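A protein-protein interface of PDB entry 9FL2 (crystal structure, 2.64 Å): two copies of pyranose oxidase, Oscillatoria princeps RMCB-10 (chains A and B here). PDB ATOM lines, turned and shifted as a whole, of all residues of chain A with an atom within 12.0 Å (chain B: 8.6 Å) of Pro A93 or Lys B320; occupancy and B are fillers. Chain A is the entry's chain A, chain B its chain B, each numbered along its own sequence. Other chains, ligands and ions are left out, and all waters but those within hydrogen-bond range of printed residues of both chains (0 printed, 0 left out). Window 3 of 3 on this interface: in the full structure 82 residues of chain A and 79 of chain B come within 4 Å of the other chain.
The backbone carbonyl oxygen (O) of Pro A93 lies within hydrogen-bond range of the side-chain amino group (NZ) of Lys B320. O of Ser A94 lies within hydrogen-bond range of N of Lys B320, 2.8 Å away. The backbone carbonyl oxygen (O) of Leu B318 sits at hydrogen-bond distance from the backbone NH (N) of Tyr A96 (2.8 Å). OH of Tyr A96 lies within hydrogen-bond range of OD2 of Asp B352, 2.6 Å away.
The side-chain hydroxyl of Ser A94 lies within hydrogen-bond range of the side-chain carboxylate of Asp A92. N of Val B317 sits at hydrogen-bond distance from O of Gly B457 (2.8 Å). The side-chain hydroxyl (OG) of Ser B319 lies close to the backbone NH (N) of Glu B321, 3.3 Å away. The backbone NH of Ile B322 is in hydrogen-bond range of the side-chain hydroxyl of Ser B319, 3.0 Å away. N of Ser B319 lies within hydrogen-bond range of O of Ile B455, at 3.0 Å.
Among the printed residues, merely in contact across the chains: Leu A91 with Val B317 (3.8 Å), Leu A91 with Phe B458 (3.8 Å), Asp A92 with Gly B457 (3.5 Å), Ser A94 with Ser B319 (3.7 Å), Ala A95 with Val B317 (3.8 Å), Ala A95 with Leu B318 (3.6 Å), Ala A95 with Lys B320 (3.2 Å), Tyr A96 with Val B317 (3.0 Å), Tyr A96 with Lys B320 (3.7 Å) and Tyr A96 with Val B323 (3.5 Å).
Pro A93 touches just one residue of chain B: Lys B320. Lys B320 touches just these residues of chain A: Pro A93 (2.9 Å), Ser A94 (2.8 Å), Ala A95 (3.2 Å) and Tyr A96 (3.7 Å). Of the printed residues of chain B, Ser A94 touches Ser B319 and Lys B320. Ser B319 touches just one residue of chain A: Ser A94 (3.7 Å). No residue of chain A comes within 4 Å of Glu B321. Val B323 touches just one residue of chain A: Tyr A96. No residue of chain A comes within 4 Å of Ala B324. Of the printed residues of chain A, Val B317 touches Leu A91, Ala A95 and Tyr A96. Of the printed residues of chain A, Gly B457 touches Asp A92 (3.5 Å). Of the printed residues of chain B, Asp A92 touches Gly B457 (3.5 Å). The nearest residue of chain B that does not touch Pro A93 is Gly B457 (7.1 Å). The nearest residue of chain A that does not touch Lys B320 is Trp A97 (5.4 Å). The nearest printed residue of chain A that does not touch Phe B458 is Asp A92 (4.8 Å).
Printed residues of chain B that touch a printed residue of chain A: Val B317, Leu B318, Ser B319, Lys B320, Val B323, Asp B352, Gly B457 and Phe B458. Along chain B the printed residues that touch a printed residue of chain A span positions 317 to 458. Of the 13 printed residues of chain A, 6 touch a printed residue of chain B. Among the printed residues, no Asp or Glu carboxylate lies within 4 Å of a Lys or Arg side-chain nitrogen of the other chain.
No position is printed for both chains.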
ATOM      1  N   LYS A  87     -20.223  15.114  15.034  1.00  0.00           N
ATOM      2  CA  LYS A  87     -20.972  13.884  14.821  1.00  0.00           C
ATOM      3  C   LYS A  87     -21.333  13.796  13.343  1.00  0.00           C
ATOM      4  O   LYS A  87     -21.902  14.738  12.795  1.00  0.00           O
ATOM      5  CB  LYS A  87     -22.202  13.805  15.728  1.00  0.00           C
ATOM      6  CG  LYS A  87     -22.838  12.436  15.748  1.00  0.00           C
ATOM      7  CD  LYS A  87     -23.921  12.300  16.807  1.00  0.00           C
ATOM      8  CE  LYS A  87     -24.659  10.991  16.787  1.00  0.00           C
ATOM      9  NZ  LYS A  87     -25.360  10.741  15.520  1.00  0.00           N
ATOM     10  N   LEU A  88     -20.973  12.679  12.699  1.00  0.00           N
ATOM     11  CA  LEU A  88     -21.194  12.516  11.274  1.00  0.00           C
ATOM     12  C   LEU A  88     -22.545  11.857  11.086  1.00  0.00           C
ATOM     13  O   LEU A  88     -22.795  10.788  11.645  1.00  0.00           O
ATOM     14  CB  LEU A  88     -20.101  11.642  10.683  1.00  0.00           C
ATOM     15  CG  LEU A  88     -18.679  12.143  10.920  1.00  0.00           C
ATOM     16  CD1 LEU A  88     -17.685  11.067  10.611  1.00  0.00           C
ATOM     17  CD2 LEU A  88     -18.439  13.365  10.071  1.00  0.00           C
ATOM     18  N   PRO A  89     -23.456  12.474  10.309  1.00  0.00           N
ATOM     19  CA  PRO A  89     -24.838  11.992  10.262  1.00  0.00           C
ATOM     20  C   PRO A  89     -25.050  10.716   9.452  1.00  0.00           C
ATOM     21  O   PRO A  89     -26.149  10.173   9.439  1.00  0.00           O
ATOM     22  CB  PRO A  89     -25.552  13.195   9.645  1.00  0.00           C
ATOM     23  CG  PRO A  89     -24.514  13.791   8.715  1.00  0.00           C
ATOM     24  CD  PRO A  89     -23.195  13.640   9.455  1.00  0.00           C
ATOM     25  N   ASN A  90     -23.977  10.215   8.822  1.00  0.00           N
ATOM     26  CA  ASN A  90     -24.080   9.245   7.743  1.00  0.00           C
ATOM     27  C   ASN A  90     -22.956   8.212   7.846  1.00  0.00           C
ATOM     28  O   ASN A  90     -22.428   7.758   6.838  1.00  0.00           O
ATOM     29  CB  ASN A  90     -24.006   9.972   6.407  1.00  0.00           C
ATOM     30  CG  ASN A  90     -22.691  10.702   6.253  1.00  0.00           C
ATOM     31  OD1 ASN A  90     -22.033  11.013   7.251  1.00  0.00           O
ATOM     32  ND2 ASN A  90     -22.268  10.969   5.028  1.00  0.00           N
ATOM     33  N   LEU A  91     -22.588   7.860   9.080  1.00  0.00           N
ATOM     34  CA  LEU A  91     -21.558   6.875   9.361  1.00  0.00           C
ATOM     35  C   LEU A  91     -22.230   5.569   9.806  1.00  0.00           C
ATOM     36  O   LEU A  91     -23.159   5.522  10.621  1.00  0.00           O
ATOM     37  CB  LEU A  91     -20.592   7.436  10.407  1.00  0.00           C
ATOM     38  CG  LEU A  91     -19.715   6.433  11.174  1.00  0.00           C
ATOM     39  CD1 LEU A  91     -18.685   5.783  10.295  1.00  0.00           C
ATOM     40  CD2 LEU A  91     -19.038   7.111  12.332  1.00  0.00           C
ATOM     41  N   ASP A  92     -21.739   4.493   9.200  1.00  0.00           N
ATOM     42  CA  ASP A  92     -22.074   3.136   9.570  1.00  0.00           C
ATOM     43  C   ASP A  92     -22.247   3.042  11.082  1.00  0.00           C
ATOM     44  O   ASP A  92     -21.327   3.346  11.835  1.00  0.00           O
ATOM     45  CB  ASP A  92     -20.948   2.242   9.069  1.00  0.00           C
ATOM     46  CG  ASP A  92     -21.248   0.761   9.003  1.00  0.00           C
ATOM     47  OD1 ASP A  92     -21.770   0.244  10.008  1.00  0.00           O
ATOM     48  OD2 ASP A  92     -20.940   0.180   7.928  1.00  0.00           O
ATOM     49  N   PRO A  93     -23.424   2.636  11.597  1.00  0.00           N
ATOM     50  CA  PRO A  93     -23.595   2.491  13.046  1.00  0.00           C
ATOM     51  C   PRO A  93     -22.789   1.358  13.683  1.00  0.00           C
ATOM     52  O   PRO A  93     -22.618   1.350  14.892  1.00  0.00           O
ATOM     53  CB  PRO A  93     -25.101   2.307  13.232  1.00  0.00           C
ATOM     54  CG  PRO A  93     -25.568   1.767  11.903  1.00  0.00           C
ATOM     55  CD  PRO A  93     -24.643   2.345  10.834  1.00  0.00           C
ATOM     56  N   SER A  94     -22.275   0.418  12.880  1.00  0.00           N
ATOM     57  CA  SER A  94     -21.382  -0.627  13.381  1.00  0.00           C
ATOM     58  C   SER A  94     -20.057  -0.030  13.844  1.00  0.00           C
ATOM     59  O   SER A  94     -19.346  -0.659  14.632  1.00  0.00           O
ATOM     60  CB  SER A  94     -21.100  -1.703  12.351  1.00  0.00           C
ATOM     61  OG  SER A  94     -20.019  -1.350  11.477  1.00  0.00           O
ATOM     62  N   ALA A  95     -19.728   1.161  13.310  1.00  0.00           N
ATOM     63  CA  ALA A  95     -18.410   1.759  13.440  1.00  0.00           C
ATOM     64  C   ALA A  95     -18.359   2.564  14.721  1.00  0.00           C
ATOM     65  O   ALA A  95     -19.361   3.123  15.143  1.00  0.00           O
ATOM     66  CB  ALA A  95     -18.067   2.614  12.227  1.00  0.00           C
ATOM     67  N   TYR A  96     -17.148   2.629  15.285  1.00  0.00           N
ATOM     68  CA  TYR A  96     -16.878   3.320  16.533  1.00  0.00           C
ATOM     69  C   TYR A  96     -16.683   4.812  16.275  1.00  0.00           C
ATOM     70  O   TYR A  96     -16.065   5.198  15.298  1.00  0.00           O
ATOM     71  CB  TYR A  96     -15.637   2.704  17.193  1.00  0.00           C
ATOM     72  CG  TYR A  96     -15.198   3.426  18.458  1.00  0.00           C
ATOM     73  CD1 TYR A  96     -15.855   3.214  19.669  1.00  0.00           C
ATOM     74  CD2 TYR A  96     -14.135   4.330  18.443  1.00  0.00           C
ATOM     75  CE1 TYR A  96     -15.467   3.875  20.826  1.00  0.00           C
ATOM     76  CE2 TYR A  96     -13.746   4.999  19.592  1.00  0.00           C
ATOM     77  CZ  TYR A  96     -14.414   4.768  20.782  1.00  0.00           C
ATOM     78  OH  TYR A  96     -14.009   5.437  21.884  1.00  0.00           O
ATOM     79  N   TRP A  97     -17.201   5.637  17.187  1.00  0.00           N
ATOM     80  CA  TRP A  97     -17.074   7.088  17.142  1.00  0.00           C
ATOM     81  C   TRP A  97     -17.039   7.638  18.574  1.00  0.00           C
ATOM     82  O   TRP A  97     -17.667   7.070  19.479  1.00  0.00           O
ATOM     83  CB  TRP A  97     -18.246   7.690  16.357  1.00  0.00           C
ATOM     84  CG  TRP A  97     -18.140   9.180  16.158  1.00  0.00           C
ATOM     85  CD1 TRP A  97     -18.724  10.161  16.902  1.00  0.00           C
ATOM     86  CD2 TRP A  97     -17.332   9.851  15.176  1.00  0.00           C
ATOM     87  NE1 TRP A  97     -18.354  11.392  16.439  1.00  0.00           N
ATOM     88  CE2 TRP A  97     -17.504  11.236  15.383  1.00  0.00           C
ATOM     89  CE3 TRP A  97     -16.486   9.416  14.153  1.00  0.00           C
ATOM     90  CZ2 TRP A  97     -16.863  12.188  14.599  1.00  0.00           C
ATOM     91  CZ3 TRP A  97     -15.857  10.362  13.368  1.00  0.00           C
ATOM     92  CH2 TRP A  97     -16.040  11.728  13.595  1.00  0.00           C
ATOM     93  N   ALA A  98     -16.309   8.752  18.764  1.00  0.00           N
ATOM     94  CA  ALA A  98     -16.341   9.493  20.017  1.00  0.00           C
ATOM     95  C   ALA A  98     -15.990  10.966  19.787  1.00  0.00           C
ATOM     96  O   ALA A  98     -14.966  11.297  19.182  1.00  0.00           O
ATOM     97  CB  ALA A  98     -15.427   8.831  21.025  1.00  0.00           C
ATOM     98  N   ALA A  99     -16.871  11.849  20.269  1.00  0.00           N
ATOM     99  CA  ALA A  99     -16.697  13.277  20.083  1.00  0.00           C
ATOM    100  C   ALA A  99     -15.852  13.835  21.216  1.00  0.00           C
ATOM    101  O   ALA A  99     -15.743  13.225  22.273  1.00  0.00           O
ATOM    102  CB  ALA A  99     -18.038  13.978  20.012  1.00  0.00           C
ATOM    103  N   ARG B 182      -9.541 -10.487  12.027  1.00  0.00           N
ATOM    104  CA  ARG B 182     -10.753 -10.410  11.229  1.00  0.00           C
ATOM    105  C   ARG B 182     -10.484 -10.775   9.770  1.00  0.00           C
ATOM    106  O   ARG B 182     -11.342 -11.363   9.122  1.00  0.00           O
ATOM    107  CB  ARG B 182     -11.390  -9.021  11.225  1.00  0.00           C
ATOM    108  CG  ARG B 182     -12.434  -8.861  12.310  1.00  0.00           C
ATOM    109  CD  ARG B 182     -11.902  -8.199  13.543  1.00  0.00           C
ATOM    110  NE  ARG B 182     -13.149  -7.756  14.178  1.00  0.00           N
ATOM    111  CZ  ARG B 182     -13.527  -8.003  15.404  1.00  0.00           C
ATOM    112  NH1 ARG B 182     -12.639  -8.426  16.294  1.00  0.00           N
ATOM    113  NH2 ARG B 182     -14.811  -7.831  15.709  1.00  0.00           N
ATOM    114  N   VAL B 317     -13.552   3.615   9.285  1.00  0.00           N
ATOM    115  CA  VAL B 317     -13.632   3.797  10.723  1.00  0.00           C
ATOM    116  C   VAL B 317     -13.783   2.416  11.356  1.00  0.00           C
ATOM    117  O   VAL B 317     -14.647   1.640  10.950  1.00  0.00           O
ATOM    118  CB  VAL B 317     -14.824   4.703  11.085  1.00  0.00           C
ATOM    119  CG1 VAL B 317     -14.860   5.066  12.559  1.00  0.00           C
ATOM    120  CG2 VAL B 317     -14.841   5.978  10.263  1.00  0.00           C
ATOM    121  N   LEU B 318     -12.951   2.132  12.368  1.00  0.00           N
ATOM    122  CA  LEU B 318     -12.878   0.812  12.975  1.00  0.00           C
ATOM    123  C   LEU B 318     -14.240   0.435  13.552  1.00  0.00           C
ATOM    124  O   LEU B 318     -14.927   1.262  14.147  1.00  0.00           O
ATOM    125  CB  LEU B 318     -11.799   0.764  14.059  1.00  0.00           C
ATOM    126  CG  LEU B 318     -10.346   0.972  13.606  1.00  0.00           C
ATOM    127  CD1 LEU B 318      -9.385   1.196  14.793  1.00  0.00           C
ATOM    128  CD2 LEU B 318      -9.845  -0.159  12.708  1.00  0.00           C
ATOM    129  N   SER B 319     -14.605  -0.841  13.387  1.00  0.00           N
ATOM    130  CA  SER B 319     -15.812  -1.390  13.977  1.00  0.00           C
ATOM    131  C   SER B 319     -15.781  -1.164  15.491  1.00  0.00           C
ATOM    132  O   SER B 319     -14.705  -1.086  16.093  1.00  0.00           O
ATOM    133  CB  SER B 319     -15.917  -2.844  13.647  1.00  0.00           C
ATOM    134  OG  SER B 319     -15.105  -3.573  14.558  1.00  0.00           O
ATOM    135  N   LYS B 320     -16.964  -1.063  16.107  1.00  0.00           N
ATOM    136  CA  LYS B 320     -17.052  -0.985  17.556  1.00  0.00           C
ATOM    137  C   LYS B 320     -16.473  -2.255  18.181  1.00  0.00           C
ATOM    138  O   LYS B 320     -15.861  -2.206  19.245  1.00  0.00           O
ATOM    139  CB  LYS B 320     -18.490  -0.767  18.040  1.00  0.00           C
ATOM    140  CG  LYS B 320     -19.053   0.623  17.789  1.00  0.00           C
ATOM    141  CD  LYS B 320     -20.515   0.770  18.178  1.00  0.00           C
ATOM    142  CE  LYS B 320     -21.114   1.984  17.557  1.00  0.00           C
ATOM    143  NZ  LYS B 320     -22.569   1.986  17.726  1.00  0.00           N
ATOM    144  N   GLU B 321     -16.672  -3.393  17.506  1.00  0.00           N
ATOM    145  CA  GLU B 321     -16.217  -4.652  18.055  1.00  0.00           C
ATOM    146  C   GLU B 321     -14.708  -4.610  18.259  1.00  0.00           C
ATOM    147  O   GLU B 321     -14.224  -4.977  19.325  1.00  0.00           O
ATOM    148  CB  GLU B 321     -16.665  -5.826  17.187  1.00  0.00           C
ATOM    149  CG  GLU B 321     -18.148  -6.153  17.390  1.00  0.00           C
ATOM    150  CD  GLU B 321     -18.454  -7.644  17.503  1.00  0.00           C
ATOM    151  OE1 GLU B 321     -17.900  -8.349  16.633  1.00  0.00           O
ATOM    152  OE2 GLU B 321     -19.182  -8.107  18.427  1.00  0.00           O
ATOM    153  N   ILE B 322     -13.983  -4.143  17.238  1.00  0.00           N
ATOM    154  CA  ILE B 322     -12.526  -4.070  17.305  1.00  0.00           C
ATOM    155  C   ILE B 322     -12.108  -3.146  18.453  1.00  0.00           C
ATOM    156  O   ILE B 322     -11.223  -3.485  19.231  1.00  0.00           O
ATOM    157  CB  ILE B 322     -11.907  -3.631  15.961  1.00  0.00           C
ATOM    158  CG1 ILE B 322     -11.916  -4.770  14.939  1.00  0.00           C
ATOM    159  CG2 ILE B 322     -10.500  -3.066  16.160  1.00  0.00           C
ATOM    160  CD1 ILE B 322     -11.397  -4.383  13.566  1.00  0.00           C
ATOM    161  N   VAL B 323     -12.732  -1.967  18.544  1.00  0.00           N
ATOM    162  CA  VAL B 323     -12.327  -1.003  19.553  1.00  0.00           C
ATOM    163  C   VAL B 323     -12.532  -1.618  20.937  1.00  0.00           C
ATOM    164  O   VAL B 323     -11.648  -1.545  21.779  1.00  0.00           O
ATOM    165  CB  VAL B 323     -13.070   0.337  19.385  1.00  0.00           C
ATOM    166  CG1 VAL B 323     -13.017   1.209  20.622  1.00  0.00           C
ATOM    167  CG2 VAL B 323     -12.553   1.116  18.183  1.00  0.00           C
ATOM    168  N   ALA B 324     -13.690  -2.247  21.158  1.00  0.00           N
ATOM    169  CA  ALA B 324     -13.967  -2.950  22.399  1.00  0.00           C
ATOM    170  C   ALA B 324     -12.799  -3.871  22.785  1.00  0.00           C
ATOM    171  O   ALA B 324     -12.366  -3.880  23.939  1.00  0.00           O
ATOM    172  CB  ALA B 324     -15.268  -3.710  22.260  1.00  0.00           C
ATOM    173  N   GLU B 325     -12.248  -4.598  21.802  1.00  0.00           N
ATOM    174  CA  GLU B 325     -11.231  -5.622  22.025  1.00  0.00           C
ATOM    175  C   GLU B 325      -9.868  -5.047  22.435  1.00  0.00           C
ATOM    176  O   GLU B 325      -8.930  -5.810  22.649  1.00  0.00           O
ATOM    177  CB  GLU B 325     -11.053  -6.401  20.716  1.00  0.00           C
ATOM    178  CG  GLU B 325     -12.076  -7.494  20.425  1.00  0.00           C
ATOM    179  CD  GLU B 325     -11.809  -8.259  19.133  1.00  0.00           C
ATOM    180  OE1 GLU B 325     -10.842  -8.049  18.336  1.00  0.00           O
ATOM    181  OE2 GLU B 325     -12.661  -9.139  18.942  1.00  0.00           O
ATOM    182  N   ILE B 326      -9.733  -3.714  22.539  1.00  0.00           N
ATOM    183  CA  ILE B 326      -8.443  -3.085  22.756  1.00  0.00           C
ATOM    184  C   ILE B 326      -8.540  -2.106  23.922  1.00  0.00           C
ATOM    185  O   ILE B 326      -9.070  -1.010  23.764  1.00  0.00           O
ATOM    186  CB  ILE B 326      -8.013  -2.387  21.458  1.00  0.00           C
ATOM    187  CG1 ILE B 326      -8.003  -3.339  20.275  1.00  0.00           C
ATOM    188  CG2 ILE B 326      -6.665  -1.705  21.631  1.00  0.00           C
ATOM    189  CD1 ILE B 326      -7.879  -2.640  18.935  1.00  0.00           C
ATOM    190  N   LYS B 327      -7.993  -2.513  25.079  1.00  0.00           N
ATOM    191  CA  LYS B 327      -8.057  -1.715  26.295  1.00  0.00           C
ATOM    192  C   LYS B 327      -6.888  -2.012  27.243  1.00  0.00           C
ATOM    193  O   LYS B 327      -7.105  -2.583  28.307  1.00  0.00           O
ATOM    194  CB  LYS B 327      -9.362  -2.114  26.993  1.00  0.00           C
ATOM    195  CG  LYS B 327     -10.641  -1.999  26.199  1.00  0.00           C
ATOM    196  CD  LYS B 327     -11.310  -0.635  26.291  1.00  0.00           C
ATOM    197  CE  LYS B 327     -12.655  -0.684  25.647  1.00  0.00           C
ATOM    198  NZ  LYS B 327     -13.600   0.204  26.322  1.00  0.00           N
ATOM    199  N   ASP B 352     -11.115   5.446  22.912  1.00  0.00           N
ATOM    200  CA  ASP B 352     -10.714   4.265  23.659  1.00  0.00           C
ATOM    201  C   ASP B 352      -9.648   3.500  22.885  1.00  0.00           C
ATOM    202  O   ASP B 352      -9.745   2.291  22.714  1.00  0.00           O
ATOM    203  CB  ASP B 352     -11.857   3.289  23.893  1.00  0.00           C
ATOM    204  CG  ASP B 352     -13.133   3.836  24.506  1.00  0.00           C
ATOM    205  OD1 ASP B 352     -13.059   4.291  25.653  1.00  0.00           O
ATOM    206  OD2 ASP B 352     -14.195   3.737  23.849  1.00  0.00           O
ATOM    207  N   ILE B 455     -13.554  -4.759   8.679  1.00  0.00           N
ATOM    208  CA  ILE B 455     -12.896  -4.213   9.857  1.00  0.00           C
ATOM    209  C   ILE B 455     -13.590  -2.939  10.327  1.00  0.00           C
ATOM    210  O   ILE B 455     -13.126  -2.319  11.268  1.00  0.00           O
ATOM    211  CB  ILE B 455     -11.396  -4.003   9.606  1.00  0.00           C
ATOM    212  CG1 ILE B 455     -11.129  -3.026   8.500  1.00  0.00           C
ATOM    213  CG2 ILE B 455     -10.717  -5.332   9.331  1.00  0.00           C
ATOM    214  CD1 ILE B 455      -9.656  -2.855   8.165  1.00  0.00           C
ATOM    215  N   GLY B 456     -14.725  -2.604   9.712  1.00  0.00           N
ATOM    216  CA  GLY B 456     -15.523  -1.459  10.117  1.00  0.00           C
ATOM    217  C   GLY B 456     -16.302  -0.914   8.923  1.00  0.00           C
ATOM    218  O   GLY B 456     -16.440  -1.613   7.920  1.00  0.00           O
ATOM    219  N   GLY B 457     -16.800   0.322   9.053  1.00  0.00           N
ATOM    220  CA  GLY B 457     -17.557   0.995   8.007  1.00  0.00           C
ATOM    221  C   GLY B 457     -16.703   2.073   7.351  1.00  0.00           C
ATOM    222  O   GLY B 457     -15.646   2.424   7.882  1.00  0.00           O
ATOM    223  N   PHE B 458     -17.148   2.583   6.197  1.00  0.00           N
ATOM    224  CA  PHE B 458     -16.338   3.562   5.498  1.00  0.00           C
ATOM    225  C   PHE B 458     -16.447   4.897   6.205  1.00  0.00           C
ATOM    226  O   PHE B 458     -17.525   5.262   6.665  1.00  0.00           O
ATOM    227  CB  PHE B 458     -16.728   3.971   4.083  1.00  0.00           C
ATOM    228  CG  PHE B 458     -16.853   2.821   3.097  1.00  0.00           C
ATOM    229  CD1 PHE B 458     -15.730   2.298   2.478  1.00  0.00           C
ATOM    230  CD2 PHE B 458     -18.104   2.314   2.752  1.00  0.00           C
ATOM    231  CE1 PHE B 458     -15.863   1.261   1.566  1.00  0.00           C
ATOM    232  CE2 PHE B 458     -18.230   1.289   1.829  1.00  0.00           C
ATOM    233  CZ  PHE B 458     -17.112   0.747   1.256  1.00  0.00           C
